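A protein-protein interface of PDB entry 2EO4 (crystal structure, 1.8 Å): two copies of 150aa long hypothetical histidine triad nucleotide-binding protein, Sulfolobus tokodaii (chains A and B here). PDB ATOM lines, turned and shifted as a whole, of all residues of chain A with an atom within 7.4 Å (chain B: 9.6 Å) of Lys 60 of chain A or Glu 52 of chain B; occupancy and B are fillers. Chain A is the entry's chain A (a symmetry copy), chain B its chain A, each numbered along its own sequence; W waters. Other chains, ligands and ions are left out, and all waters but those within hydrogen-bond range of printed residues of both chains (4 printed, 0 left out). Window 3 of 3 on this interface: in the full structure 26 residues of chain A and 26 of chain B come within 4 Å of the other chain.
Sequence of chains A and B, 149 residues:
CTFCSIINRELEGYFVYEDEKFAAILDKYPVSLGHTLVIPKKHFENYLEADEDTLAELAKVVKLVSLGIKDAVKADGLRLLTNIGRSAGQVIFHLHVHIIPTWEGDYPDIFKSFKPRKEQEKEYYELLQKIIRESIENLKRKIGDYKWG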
ATOM      1  N   TYR A  17       9.094   8.839  21.049  1.00  0.00           N
ATOM      2  CA  TYR A  17       8.014   8.198  20.306  1.00  0.00           C
ATOM      3  C   TYR A  17       7.727   8.972  19.031  1.00  0.00           C
ATOM      4  O   TYR A  17       7.768  10.203  19.010  1.00  0.00           O
ATOM      5  CB  TYR A  17       6.714   8.131  21.120  1.00  0.00           C
ATOM      6  CG  TYR A  17       5.561   7.540  20.326  1.00  0.00           C
ATOM      7  CD1 TYR A  17       5.377   6.162  20.251  1.00  0.00           C
ATOM      8  CD2 TYR A  17       4.691   8.360  19.602  1.00  0.00           C
ATOM      9  CE1 TYR A  17       4.359   5.608  19.475  1.00  0.00           C
ATOM     10  CE2 TYR A  17       3.667   7.818  18.818  1.00  0.00           C
ATOM     11  CZ  TYR A  17       3.510   6.441  18.762  1.00  0.00           C
ATOM     12  OH  TYR A  17       2.507   5.892  17.992  1.00  0.00           O
ATOM     13  N   VAL A  38       3.812  15.351  24.358  1.00  0.00           N
ATOM     14  CA  VAL A  38       3.239  14.549  23.284  1.00  0.00           C
ATOM     15  C   VAL A  38       2.559  15.535  22.355  1.00  0.00           C
ATOM     16  O   VAL A  38       1.754  16.360  22.791  1.00  0.00           O
ATOM     17  CB  VAL A  38       2.201  13.541  23.809  1.00  0.00           C
ATOM     18  CG1 VAL A  38       1.664  12.705  22.651  1.00  0.00           C
ATOM     19  CG2 VAL A  38       2.839  12.643  24.859  1.00  0.00           C
ATOM     20  N   ASP A  53     -10.624  13.778  15.271  1.00  0.00           N
ATOM     21  CA  ASP A  53      -9.807  12.608  14.970  1.00  0.00           C
ATOM     22  C   ASP A  53      -8.391  12.768  15.523  1.00  0.00           C
ATOM     23  O   ASP A  53      -7.795  11.808  16.010  1.00  0.00           O
ATOM     24  CB  ASP A  53      -9.761  12.348  13.462  1.00  0.00           C
ATOM     25  CG  ASP A  53     -11.103  11.912  12.909  1.00  0.00           C
ATOM     26  OD1 ASP A  53     -11.864  11.248  13.647  1.00  0.00           O
ATOM     27  OD2 ASP A  53     -11.391  12.228  11.736  1.00  0.00           O
ATOM     28  N   THR A  54      -7.854  13.979  15.446  1.00  0.00           N
ATOM     29  CA  THR A  54      -6.521  14.237  15.975  1.00  0.00           C
ATOM     30  C   THR A  54      -6.535  14.088  17.497  1.00  0.00           C
ATOM     31  O   THR A  54      -5.642  13.470  18.077  1.00  0.00           O
ATOM     32  CB  THR A  54      -6.036  15.661  15.622  1.00  0.00           C
ATOM     33  OG1 THR A  54      -5.839  15.765  14.207  1.00  0.00           O
ATOM     34  CG2 THR A  54      -4.716  15.966  16.322  1.00  0.00           C
ATOM     35  N   LEU A  55      -7.551  14.658  18.138  1.00  0.00           N
ATOM     36  CA  LEU A  55      -7.658  14.583  19.594  1.00  0.00           C
ATOM     37  C   LEU A  55      -7.840  13.148  20.074  1.00  0.00           C
ATOM     38  O   LEU A  55      -7.298  12.757  21.109  1.00  0.00           O
ATOM     39  CB  LEU A  55      -8.823  15.449  20.092  1.00  0.00           C
ATOM     40  CG  LEU A  55      -8.657  16.964  19.942  1.00  0.00           C
ATOM     41  CD1 LEU A  55      -9.882  17.673  20.501  1.00  0.00           C
ATOM     42  CD2 LEU A  55      -7.404  17.423  20.684  1.00  0.00           C
ATOM     43  N   ALA A  56      -8.600  12.361  19.319  1.00  0.00           N
ATOM     44  CA  ALA A  56      -8.841  10.970  19.685  1.00  0.00           C
ATOM     45  C   ALA A  56      -7.554  10.157  19.636  1.00  0.00           C
ATOM     46  O   ALA A  56      -7.258   9.390  20.556  1.00  0.00           O
ATOM     47  CB  ALA A  56      -9.888  10.355  18.750  1.00  0.00           C
ATOM     48  N   GLU A  57      -6.789  10.321  18.563  1.00  0.00           N
ATOM     49  CA  GLU A  57      -5.539   9.586  18.421  1.00  0.00           C
ATOM     50  C   GLU A  57      -4.502  10.114  19.405  1.00  0.00           C
ATOM     51  O   GLU A  57      -3.681   9.356  19.916  1.00  0.00           O
ATOM     52  CB  GLU A  57      -5.014   9.703  16.988  1.00  0.00           C
ATOM     53  CG  GLU A  57      -3.794   8.837  16.698  1.00  0.00           C
ATOM     54  CD  GLU A  57      -3.984   7.384  17.110  1.00  0.00           C
ATOM     55  OE1 GLU A  57      -5.072   6.820  16.849  1.00  0.00           O
ATOM     56  OE2 GLU A  57      -3.038   6.803  17.688  1.00  0.00           O
ATOM     57  N   LEU A  58      -4.543  11.419  19.665  1.00  0.00           N
ATOM     58  CA  LEU A  58      -3.613  12.035  20.608  1.00  0.00           C
ATOM     59  C   LEU A  58      -3.790  11.389  21.982  1.00  0.00           C
ATOM     60  O   LEU A  58      -2.818  11.082  22.670  1.00  0.00           O
ATOM     61  CB  LEU A  58      -3.884  13.541  20.710  1.00  0.00           C
ATOM     62  CG  LEU A  58      -3.066  14.323  21.747  1.00  0.00           C
ATOM     63  CD1 LEU A  58      -1.588  14.229  21.414  1.00  0.00           C
ATOM     64  CD2 LEU A  58      -3.514  15.782  21.767  1.00  0.00           C
ATOM     65  N   ALA A  59      -5.040  11.180  22.376  1.00  0.00           N
ATOM     66  CA  ALA A  59      -5.327  10.574  23.673  1.00  0.00           C
ATOM     67  C   ALA A  59      -4.723   9.175  23.777  1.00  0.00           C
ATOM     68  O   ALA A  59      -4.227   8.780  24.831  1.00  0.00           O
ATOM     69  CB  ALA A  59      -6.831  10.508  23.901  1.00  0.00           C
ATOM     70  N   LYS A  60      -4.777   8.428  22.678  1.00  0.00           N
ATOM     71  CA  LYS A  60      -4.239   7.072  22.652  1.00  0.00           C
ATOM     72  C   LYS A  60      -2.716   7.075  22.729  1.00  0.00           C
ATOM     73  O   LYS A  60      -2.115   6.221  23.386  1.00  0.00           O
ATOM     74  CB  LYS A  60      -4.708   6.353  21.382  1.00  0.00           C
ATOM     75  CG  LYS A  60      -6.219   6.226  21.296  1.00  0.00           C
ATOM     76  CD  LYS A  60      -6.663   5.572  19.998  1.00  0.00           C
ATOM     77  CE  LYS A  60      -8.180   5.603  19.873  1.00  0.00           C
ATOM     78  NZ  LYS A  60      -8.656   4.955  18.619  1.00  0.00           N
ATOM     79  N   VAL A  61      -2.088   8.032  22.052  1.00  0.00           N
ATOM     80  CA  VAL A  61      -0.636   8.136  22.080  1.00  0.00           C
ATOM     81  C   VAL A  61      -0.201   8.540  23.489  1.00  0.00           C
ATOM     82  O   VAL A  61       0.777   8.020  24.022  1.00  0.00           O
ATOM     83  CB  VAL A  61      -0.125   9.182  21.056  1.00  0.00           C
ATOM     84  CG1 VAL A  61       1.365   9.414  21.242  1.00  0.00           C
ATOM     85  CG2 VAL A  61      -0.403   8.696  19.635  1.00  0.00           C
ATOM     86  N   VAL A  62      -0.936   9.467  24.094  1.00  0.00           N
ATOM     87  CA  VAL A  62      -0.622   9.909  25.448  1.00  0.00           C
ATOM     88  C   VAL A  62      -0.653   8.714  26.409  1.00  0.00           C
ATOM     89  O   VAL A  62       0.213   8.580  27.273  1.00  0.00           O
ATOM     90  CB  VAL A  62      -1.617  10.999  25.915  1.00  0.00           C
ATOM     91  CG1 VAL A  62      -1.465  11.260  27.414  1.00  0.00           C
ATOM     92  CG2 VAL A  62      -1.347  12.284  25.151  1.00  0.00           C
ATOM     93  N   LYS A  63      -1.634   7.831  26.253  1.00  0.00           N
ATOM     94  CA  LYS A  63      -1.693   6.661  27.136  1.00  0.00           C
ATOM     95  C   LYS A  63      -0.443   5.791  26.977  1.00  0.00           C
ATOM     96  O   LYS A  63       0.207   5.434  27.959  1.00  0.00           O
ATOM     97  CB  LYS A  63      -2.928   5.800  26.848  1.00  0.00           C
ATOM     98  CG  LYS A  63      -2.983   4.541  27.728  1.00  0.00           C
ATOM     99  CD  LYS A  63      -4.190   3.651  27.435  1.00  0.00           C
ATOM    100  CE  LYS A  63      -4.124   2.372  28.268  1.00  0.00           C
ATOM    101  NZ  LYS A  63      -5.320   1.489  28.095  1.00  0.00           N
ATOM    102  N   LEU A  64      -0.118   5.440  25.736  1.00  0.00           N
ATOM    103  CA  LEU A  64       1.048   4.602  25.467  1.00  0.00           C
ATOM    104  C   LEU A  64       2.340   5.201  26.012  1.00  0.00           C
ATOM    105  O   LEU A  64       3.096   4.539  26.730  1.00  0.00           O
ATOM    106  CB  LEU A  64       1.202   4.369  23.960  1.00  0.00           C
ATOM    107  CG  LEU A  64       2.492   3.662  23.527  1.00  0.00           C
ATOM    108  CD1 LEU A  64       2.569   2.291  24.181  1.00  0.00           C
ATOM    109  CD2 LEU A  64       2.529   3.535  22.008  1.00  0.00           C
ATOM    110  N   VAL A  65       2.597   6.458  25.665  1.00  0.00           N
ATOM    111  CA  VAL A  65       3.808   7.121  26.116  1.00  0.00           C
ATOM    112  C   VAL A  65       3.844   7.246  27.637  1.00  0.00           C
ATOM    113  O   VAL A  65       4.898   7.074  28.245  1.00  0.00           O
ATOM    114  CB  VAL A  65       3.952   8.509  25.458  1.00  0.00           C
ATOM    115  CG1 VAL A  65       5.190   9.225  25.995  1.00  0.00           C
ATOM    116  CG2 VAL A  65       4.058   8.339  23.944  1.00  0.00           C
ATOM    117  N   SER A  66       2.697   7.535  28.248  1.00  0.00           N
ATOM    118  CA  SER A  66       2.631   7.656  29.702  1.00  0.00           C
ATOM    119  C   SER A  66       2.993   6.316  30.346  1.00  0.00           C
ATOM    120  O   SER A  66       3.768   6.268  31.302  1.00  0.00           O
ATOM    121  CB  SER A  66       1.230   8.089  30.152  1.00  0.00           C
ATOM    122  OG  SER A  66       0.951   9.428  29.758  1.00  0.00           O
ATOM    123  N   ILE A 143       1.252  -5.595  24.533  1.00  0.00           N
ATOM    124  CA  ILE A 143      -0.113  -5.082  24.425  1.00  0.00           C
ATOM    125  C   ILE A 143      -0.358  -4.354  23.104  1.00  0.00           C
ATOM    126  O   ILE A 143      -1.375  -3.682  22.938  1.00  0.00           O
ATOM    127  CB  ILE A 143      -0.458  -4.113  25.591  1.00  0.00           C
ATOM    128  CG1 ILE A 143       0.300  -2.793  25.429  1.00  0.00           C
ATOM    129  CG2 ILE A 143      -0.111  -4.761  26.927  1.00  0.00           C
ATOM    130  CD1 ILE A 143      -0.068  -1.739  26.454  1.00  0.00           C
ATOM    131  N   ASP A 145      -0.723  -4.048  18.754  1.00  0.00           N
ATOM    132  CA  ASP A 145      -1.615  -4.669  17.777  1.00  0.00           C
ATOM    133  C   ASP A 145      -1.108  -6.043  17.357  1.00  0.00           C
ATOM    134  O   ASP A 145      -1.875  -6.885  16.888  1.00  0.00           O
ATOM    135  CB  ASP A 145      -1.746  -3.786  16.531  1.00  0.00           C
ATOM    136  CG  ASP A 145      -2.363  -2.437  16.833  1.00  0.00           C
ATOM    137  OD1 ASP A 145      -3.493  -2.405  17.364  1.00  0.00           O
ATOM    138  OD2 ASP A 145      -1.719  -1.409  16.534  1.00  0.00           O
ATOM    139  N   PHE B  22     -20.824   9.541  29.029  1.00  0.00           N
ATOM    140  CA  PHE B  22     -20.013  10.580  29.660  1.00  0.00           C
ATOM    141  C   PHE B  22     -20.842  11.659  30.331  1.00  0.00           C
ATOM    142  O   PHE B  22     -22.048  11.765  30.113  1.00  0.00           O
ATOM    143  CB  PHE B  22     -19.093  11.236  28.626  1.00  0.00           C
ATOM    144  CG  PHE B  22     -18.106  10.290  28.013  1.00  0.00           C
ATOM    145  CD1 PHE B  22     -18.492   9.424  26.994  1.00  0.00           C
ATOM    146  CD2 PHE B  22     -16.798  10.234  28.485  1.00  0.00           C
ATOM    147  CE1 PHE B  22     -17.586   8.513  26.455  1.00  0.00           C
ATOM    148  CE2 PHE B  22     -15.883   9.326  27.952  1.00  0.00           C
ATOM    149  CZ  PHE B  22     -16.278   8.462  26.936  1.00  0.00           C
ATOM    150  N   PHE B  44     -13.072   3.901  36.031  1.00  0.00           N
ATOM    151  CA  PHE B  44     -11.682   3.557  35.725  1.00  0.00           C
ATOM    152  C   PHE B  44     -10.878   4.298  36.790  1.00  0.00           C
ATOM    153  O   PHE B  44     -11.144   5.466  37.060  1.00  0.00           O
ATOM    154  CB  PHE B  44     -11.269   4.060  34.334  1.00  0.00           C
ATOM    155  CG  PHE B  44     -11.924   3.326  33.202  1.00  0.00           C
ATOM    156  CD1 PHE B  44     -11.594   2.001  32.931  1.00  0.00           C
ATOM    157  CD2 PHE B  44     -12.866   3.961  32.401  1.00  0.00           C
ATOM    158  CE1 PHE B  44     -12.195   1.320  31.873  1.00  0.00           C
ATOM    159  CE2 PHE B  44     -13.473   3.290  31.341  1.00  0.00           C
ATOM    160  CZ  PHE B  44     -13.134   1.967  31.078  1.00  0.00           C
ATOM    161  N   TYR B  47      -6.456   7.572  34.140  1.00  0.00           N
ATOM    162  CA  TYR B  47      -6.313   7.646  32.688  1.00  0.00           C
ATOM    163  C   TYR B  47      -5.689   6.399  32.055  1.00  0.00           C
ATOM    164  O   TYR B  47      -6.107   5.960  30.983  1.00  0.00           O
ATOM    165  CB  TYR B  47      -5.472   8.885  32.344  1.00  0.00           C
ATOM    166  CG  TYR B  47      -5.450   9.269  30.879  1.00  0.00           C
ATOM    167  CD1 TYR B  47      -4.566   8.666  29.986  1.00  0.00           C
ATOM    168  CD2 TYR B  47      -6.305  10.258  30.393  1.00  0.00           C
ATOM    169  CE1 TYR B  47      -4.527   9.041  28.644  1.00  0.00           C
ATOM    170  CE2 TYR B  47      -6.276  10.641  29.053  1.00  0.00           C
ATOM    171  CZ  TYR B  47      -5.387  10.032  28.187  1.00  0.00           C
ATOM    172  OH  TYR B  47      -5.358  10.415  26.867  1.00  0.00           O
ATOM    173  N   LEU B  48      -4.696   5.831  32.725  1.00  0.00           N
ATOM    174  CA  LEU B  48      -3.992   4.661  32.208  1.00  0.00           C
ATOM    175  C   LEU B  48      -4.800   3.366  32.210  1.00  0.00           C
ATOM    176  O   LEU B  48      -4.462   2.420  31.492  1.00  0.00           O
ATOM    177  CB  LEU B  48      -2.699   4.455  32.999  1.00  0.00           C
ATOM    178  CG  LEU B  48      -1.800   5.694  33.099  1.00  0.00           C
ATOM    179  CD1 LEU B  48      -0.564   5.358  33.910  1.00  0.00           C
ATOM    180  CD2 LEU B  48      -1.413   6.174  31.706  1.00  0.00           C
ATOM    181  N   GLU B  49      -5.858   3.320  33.010  1.00  0.00           N
ATOM    182  CA  GLU B  49      -6.684   2.115  33.102  1.00  0.00           C
ATOM    183  C   GLU B  49      -7.854   2.095  32.127  1.00  0.00           C
ATOM    184  O   GLU B  49      -8.524   1.073  31.977  1.00  0.00           O
ATOM    185  CB  GLU B  49      -7.217   1.949  34.529  1.00  0.00           C
ATOM    186  CG  GLU B  49      -6.148   1.727  35.585  1.00  0.00           C
ATOM    187  CD  GLU B  49      -5.328   0.480  35.333  1.00  0.00           C
ATOM    188  OE1 GLU B  49      -5.922  -0.555  34.963  1.00  0.00           O
ATOM    189  OE2 GLU B  49      -4.091   0.531  35.516  1.00  0.00           O
ATOM    190  N   ALA B  50      -8.098   3.217  31.458  1.00  0.00           N
ATOM    191  CA  ALA B  50      -9.201   3.309  30.511  1.00  0.00           C
ATOM    192  C   ALA B  50      -8.823   2.750  29.142  1.00  0.00           C
ATOM    193  O   ALA B  50      -7.675   2.864  28.716  1.00  0.00           O
ATOM    194  CB  ALA B  50      -9.644   4.763  30.371  1.00  0.00           C
ATOM    195  N   ASP B  51      -9.795   2.147  28.462  1.00  0.00           N
ATOM    196  CA  ASP B  51      -9.559   1.592  27.129  1.00  0.00           C
ATOM    197  C   ASP B  51      -9.442   2.748  26.138  1.00  0.00           C
ATOM    198  O   ASP B  51      -9.872   3.865  26.426  1.00  0.00           O
ATOM    199  CB  ASP B  51     -10.714   0.676  26.712  1.00  0.00           C
ATOM    200  CG  ASP B  51     -12.041   1.404  26.659  1.00  0.00           C
ATOM    201  OD1 ASP B  51     -12.639   1.633  27.729  1.00  0.00           O
ATOM    202  OD2 ASP B  51     -12.481   1.762  25.546  1.00  0.00           O
ATOM    203  N   GLU B  52      -8.874   2.477  24.966  1.00  0.00           N
ATOM    204  CA  GLU B  52      -8.685   3.513  23.954  1.00  0.00           C
ATOM    205  C   GLU B  52      -9.961   4.171  23.439  1.00  0.00           C
ATOM    206  O   GLU B  52      -9.973   5.375  23.182  1.00  0.00           O
ATOM    207  CB  GLU B  52      -7.884   2.958  22.772  1.00  0.00           C
ATOM    208  CG  GLU B  52      -6.488   2.490  23.142  1.00  0.00           C
ATOM    209  CD  GLU B  52      -5.634   2.189  21.925  1.00  0.00           C
ATOM    210  OE1 GLU B  52      -6.140   1.542  20.987  1.00  0.00           O
ATOM    211  OE2 GLU B  52      -4.455   2.593  21.910  1.00  0.00           O
ATOM    212  N   ASP B  53     -11.033   3.401  23.278  1.00  0.00           N
ATOM    213  CA  ASP B  53     -12.281   3.980  22.791  1.00  0.00           C
ATOM    214  C   ASP B  53     -12.848   4.986  23.792  1.00  0.00           C
ATOM    215  O   ASP B  53     -13.390   6.020  23.404  1.00  0.00           O
ATOM    216  CB  ASP B  53     -13.311   2.887  22.495  1.00  0.00           C
ATOM    217  CG  ASP B  53     -12.914   2.022  21.315  1.00  0.00           C
ATOM    218  OD1 ASP B  53     -12.256   2.545  20.388  1.00  0.00           O
ATOM    219  OD2 ASP B  53     -13.268   0.825  21.313  1.00  0.00           O
ATOM    220  N   THR B  54     -12.726   4.681  25.078  1.00  0.00           N
ATOM    221  CA  THR B  54     -13.209   5.592  26.108  1.00  0.00           C
ATOM    222  C   THR B  54     -12.372   6.872  26.094  1.00  0.00           C
ATOM    223  O   THR B  54     -12.910   7.977  26.162  1.00  0.00           O
ATOM    224  CB  THR B  54     -13.119   4.959  27.514  1.00  0.00           C
ATOM    225  OG1 THR B  54     -14.037   3.862  27.607  1.00  0.00           O
ATOM    226  CG2 THR B  54     -13.471   5.983  28.586  1.00  0.00           C
ATOM    227  N   LEU B  55     -11.054   6.717  26.005  1.00  0.00           N
ATOM    228  CA  LEU B  55     -10.160   7.874  25.991  1.00  0.00           C
ATOM    229  C   LEU B  55     -10.386   8.748  24.764  1.00  0.00           C
ATOM    230  O   LEU B  55     -10.320   9.976  24.844  1.00  0.00           O
ATOM    231  CB  LEU B  55      -8.695   7.420  26.044  1.00  0.00           C
ATOM    232  CG  LEU B  55      -8.229   6.773  27.352  1.00  0.00           C
ATOM    233  CD1 LEU B  55      -6.756   6.405  27.246  1.00  0.00           C
ATOM    234  CD2 LEU B  55      -8.444   7.742  28.512  1.00  0.00           C
ATOM    235  N   ALA B  56     -10.658   8.115  23.627  1.00  0.00           N
ATOM    236  CA  ALA B  56     -10.892   8.854  22.391  1.00  0.00           C
ATOM    237  C   ALA B  56     -12.153   9.702  22.486  1.00  0.00           C
ATOM    238  O   ALA B  56     -12.152  10.878  22.111  1.00  0.00           O
ATOM    239  CB  ALA B  56     -10.999   7.883  21.211  1.00  0.00           C
ATOM    240  N   GLU B  57     -13.231   9.109  22.987  1.00  0.00           N
ATOM    241  CA  GLU B  57     -14.487   9.834  23.117  1.00  0.00           C
ATOM    242  C   GLU B  57     -14.383  10.875  24.225  1.00  0.00           C
ATOM    243  O   GLU B  57     -14.975  11.949  24.134  1.00  0.00           O
ATOM    244  CB  GLU B  57     -15.634   8.864  23.411  1.00  0.00           C
ATOM    245  CG  GLU B  57     -17.014   9.509  23.407  1.00  0.00           C
ATOM    246  CD  GLU B  57     -17.283  10.332  22.155  1.00  0.00           C
ATOM    247  OE1 GLU B  57     -16.944   9.866  21.043  1.00  0.00           O
ATOM    248  OE2 GLU B  57     -17.842  11.444  22.285  1.00  0.00           O
ATOM    249  N   LEU B  58     -13.628  10.551  25.273  1.00  0.00           N
ATOM    250  CA  LEU B  58     -13.437  11.478  26.386  1.00  0.00           C
ATOM    251  C   LEU B  58     -12.794  12.763  25.865  1.00  0.00           C
ATOM    252  O   LEU B  58     -13.186  13.867  26.238  1.00  0.00           O
ATOM    253  CB  LEU B  58     -12.530  10.846  27.449  1.00  0.00           C
ATOM    254  CG  LEU B  58     -12.134  11.733  28.638  1.00  0.00           C
ATOM    255  CD1 LEU B  58     -13.375  12.152  29.403  1.00  0.00           C
ATOM    256  CD2 LEU B  58     -11.175  10.976  29.552  1.00  0.00           C
ATOM    257  N   ALA B  59     -11.805  12.613  24.992  1.00  0.00           N
ATOM    258  CA  ALA B  59     -11.116  13.773  24.433  1.00  0.00           C
ATOM    259  C   ALA B  59     -12.081  14.675  23.667  1.00  0.00           C
ATOM    260  O   ALA B  59     -11.974  15.899  23.718  1.00  0.00           O
ATOM    261  CB  ALA B  59      -9.989  13.321  23.515  1.00  0.00           C
ATOM    262  N   LYS B  60     -13.018  14.060  22.950  1.00  0.00           N
ATOM    263  CA  LYS B  60     -13.996  14.812  22.171  1.00  0.00           C
ATOM    264  C   LYS B  60     -14.984  15.543  23.071  1.00  0.00           C
ATOM    265  O   LYS B  60     -15.383  16.675  22.785  1.00  0.00           O
ATOM    266  CB  LYS B  60     -14.738  13.866  21.220  1.00  0.00           C
ATOM    267  CG  LYS B  60     -13.817  13.182  20.225  1.00  0.00           C
ATOM    268  CD  LYS B  60     -14.564  12.198  19.340  1.00  0.00           C
ATOM    269  CE  LYS B  60     -13.592  11.417  18.465  1.00  0.00           C
ATOM    270  NZ  LYS B  60     -14.290  10.453  17.569  1.00  0.00           N
ATOM    271  N   LEU B  95     -11.454   8.220  36.895  1.00  0.00           N
ATOM    272  CA  LEU B  95     -10.910   9.074  35.845  1.00  0.00           C
ATOM    273  C   LEU B  95     -11.734  10.318  35.558  1.00  0.00           C
ATOM    274  O   LEU B  95     -12.913  10.235  35.220  1.00  0.00           O
ATOM    275  CB  LEU B  95     -10.749   8.263  34.552  1.00  0.00           C
ATOM    276  CG  LEU B  95     -10.394   9.000  33.252  1.00  0.00           C
ATOM    277  CD1 LEU B  95      -9.144   9.849  33.420  1.00  0.00           C
ATOM    278  CD2 LEU B  95     -10.195   7.965  32.153  1.00  0.00           C
HETATM  279  O   HOH W   1     -12.035   9.247  15.852  1.00  0.00           O
HETATM  280  O   HOH W   2     -11.727   5.039  18.840  1.00  0.00           O
HETATM  281  O   HOH W   3      -8.103   1.980  19.360  1.00  0.00           O
HETATM  282  O   HOH W   4      -2.919   3.734  23.987  1.00  0.00           O
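The side-chain hydroxyl (OH) of Tyr 47 of chain B lies within hydrogen-bond range of the backbone carbonyl oxygen (O) of Ala 59 of chain A, at 2.8 Å.
The side-chain amino group (NZ) of Lys 63 of chain A lies within hydrogen-bond range of the backbone carbonyl oxygen (O) of Ala 50 of chain B (2.8 Å).
O of Val 62 of chain A lies within hydrogen-bond range of OG of Ser 66 of chain A (2.7 Å).
Among the printed residues, pairs that only touch across the chains: Lys 63 of chain A with Leu 48 of chain B, Ser 66 of chain A with Leu 48 of chain B, Ala 59 of chain A with Leu 55 of chain B, Leu 55 of chain A with Ala 59 of chain B, Ala 56 of chain A with Ala 56 of chain B, Lys 63 of chain A with Leu 55 of chain B, Lys 60 of chain A with Glu 52 of chain B, Ala 56 of chain A with Lys 60 of chain B, Lys 60 of chain A with Ala 56 of chain B, Val 62 of chain A with Tyr 47 of chain B and Lys 63 of chain A with Tyr 47 of chain B.
Thr 54 of chain A touches none of the printed residues of chain B.
No residue of chain B comes within 4 Å of Glu 57 of chain A.
Lys 60 of chain A touches two residues of chain B.
Printed residues of chain B within 4 Å of Lys 63 of chain A: Tyr 47, Leu 48, Ala 50 and Leu 55.
Of the printed residues of chain B, Ser 66 of chain A touches Leu 48 (3.6 Å).
Of chain A, only Lys 60 comes within 4 Å of Glu 52 of chain B.
Of the 17 printed residues of chain B, 8 touch a printed residue of chain A.
Printed residues of chain B that touch a printed residue of chain A: Tyr 47, Leu 48, Ala 50, Glu 52, Leu 55, Ala 56, Ala 59 and Lys 60.
Of the 18 printed residues of chain A, 7 touch a printed residue of chain B.
Printed residues of chain A that touch a printed residue of chain B: Leu 55, Ala 56, Ala 59, Lys 60, Val 62, Lys 63 and Ser 66.
Leu 55 of chain A touches Ala 59 of chain B, and with the chains exchanged Ala 59 of chain A touches Leu 55 of chain B.
Ala 56 of chain B touches its own counterpart, Ala 56 of chain A.
Ala 56 of chain A touches Lys 60 of chain B, and with the chains exchanged Lys 60 of chain A touches Ala 56 of chain B.
Positions printed for both chains: 53, 54, 55, 56, 57, 58, 59 and 60.
Of the 13 pairs that touch across the chains among the printed residues, 5 have their exchanged pair printed and touching as well.
Water W3 bridges OE1 of Glu 52 of chain B (2.6 Å) and NZ of Lys 60 of chain A (3.1 Å).
Water W4 bridges the backbone carbonyl oxygen (O) of Lys 60 of chain A (2.7 Å) and the side-chain carboxylate (OE2) of Glu 52 of chain B (2.8 Å).
Water W2 lies within hydrogen-bond range of OD1 of Asp 53 of chain B (3.0 Å) and NZ of Lys 60 of chain A (3.1 Å).
Water W1 bridges OD1 of Asp 53 of chain A (3.0 Å) and NZ of Lys 60 of chain B (3.1 Å).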
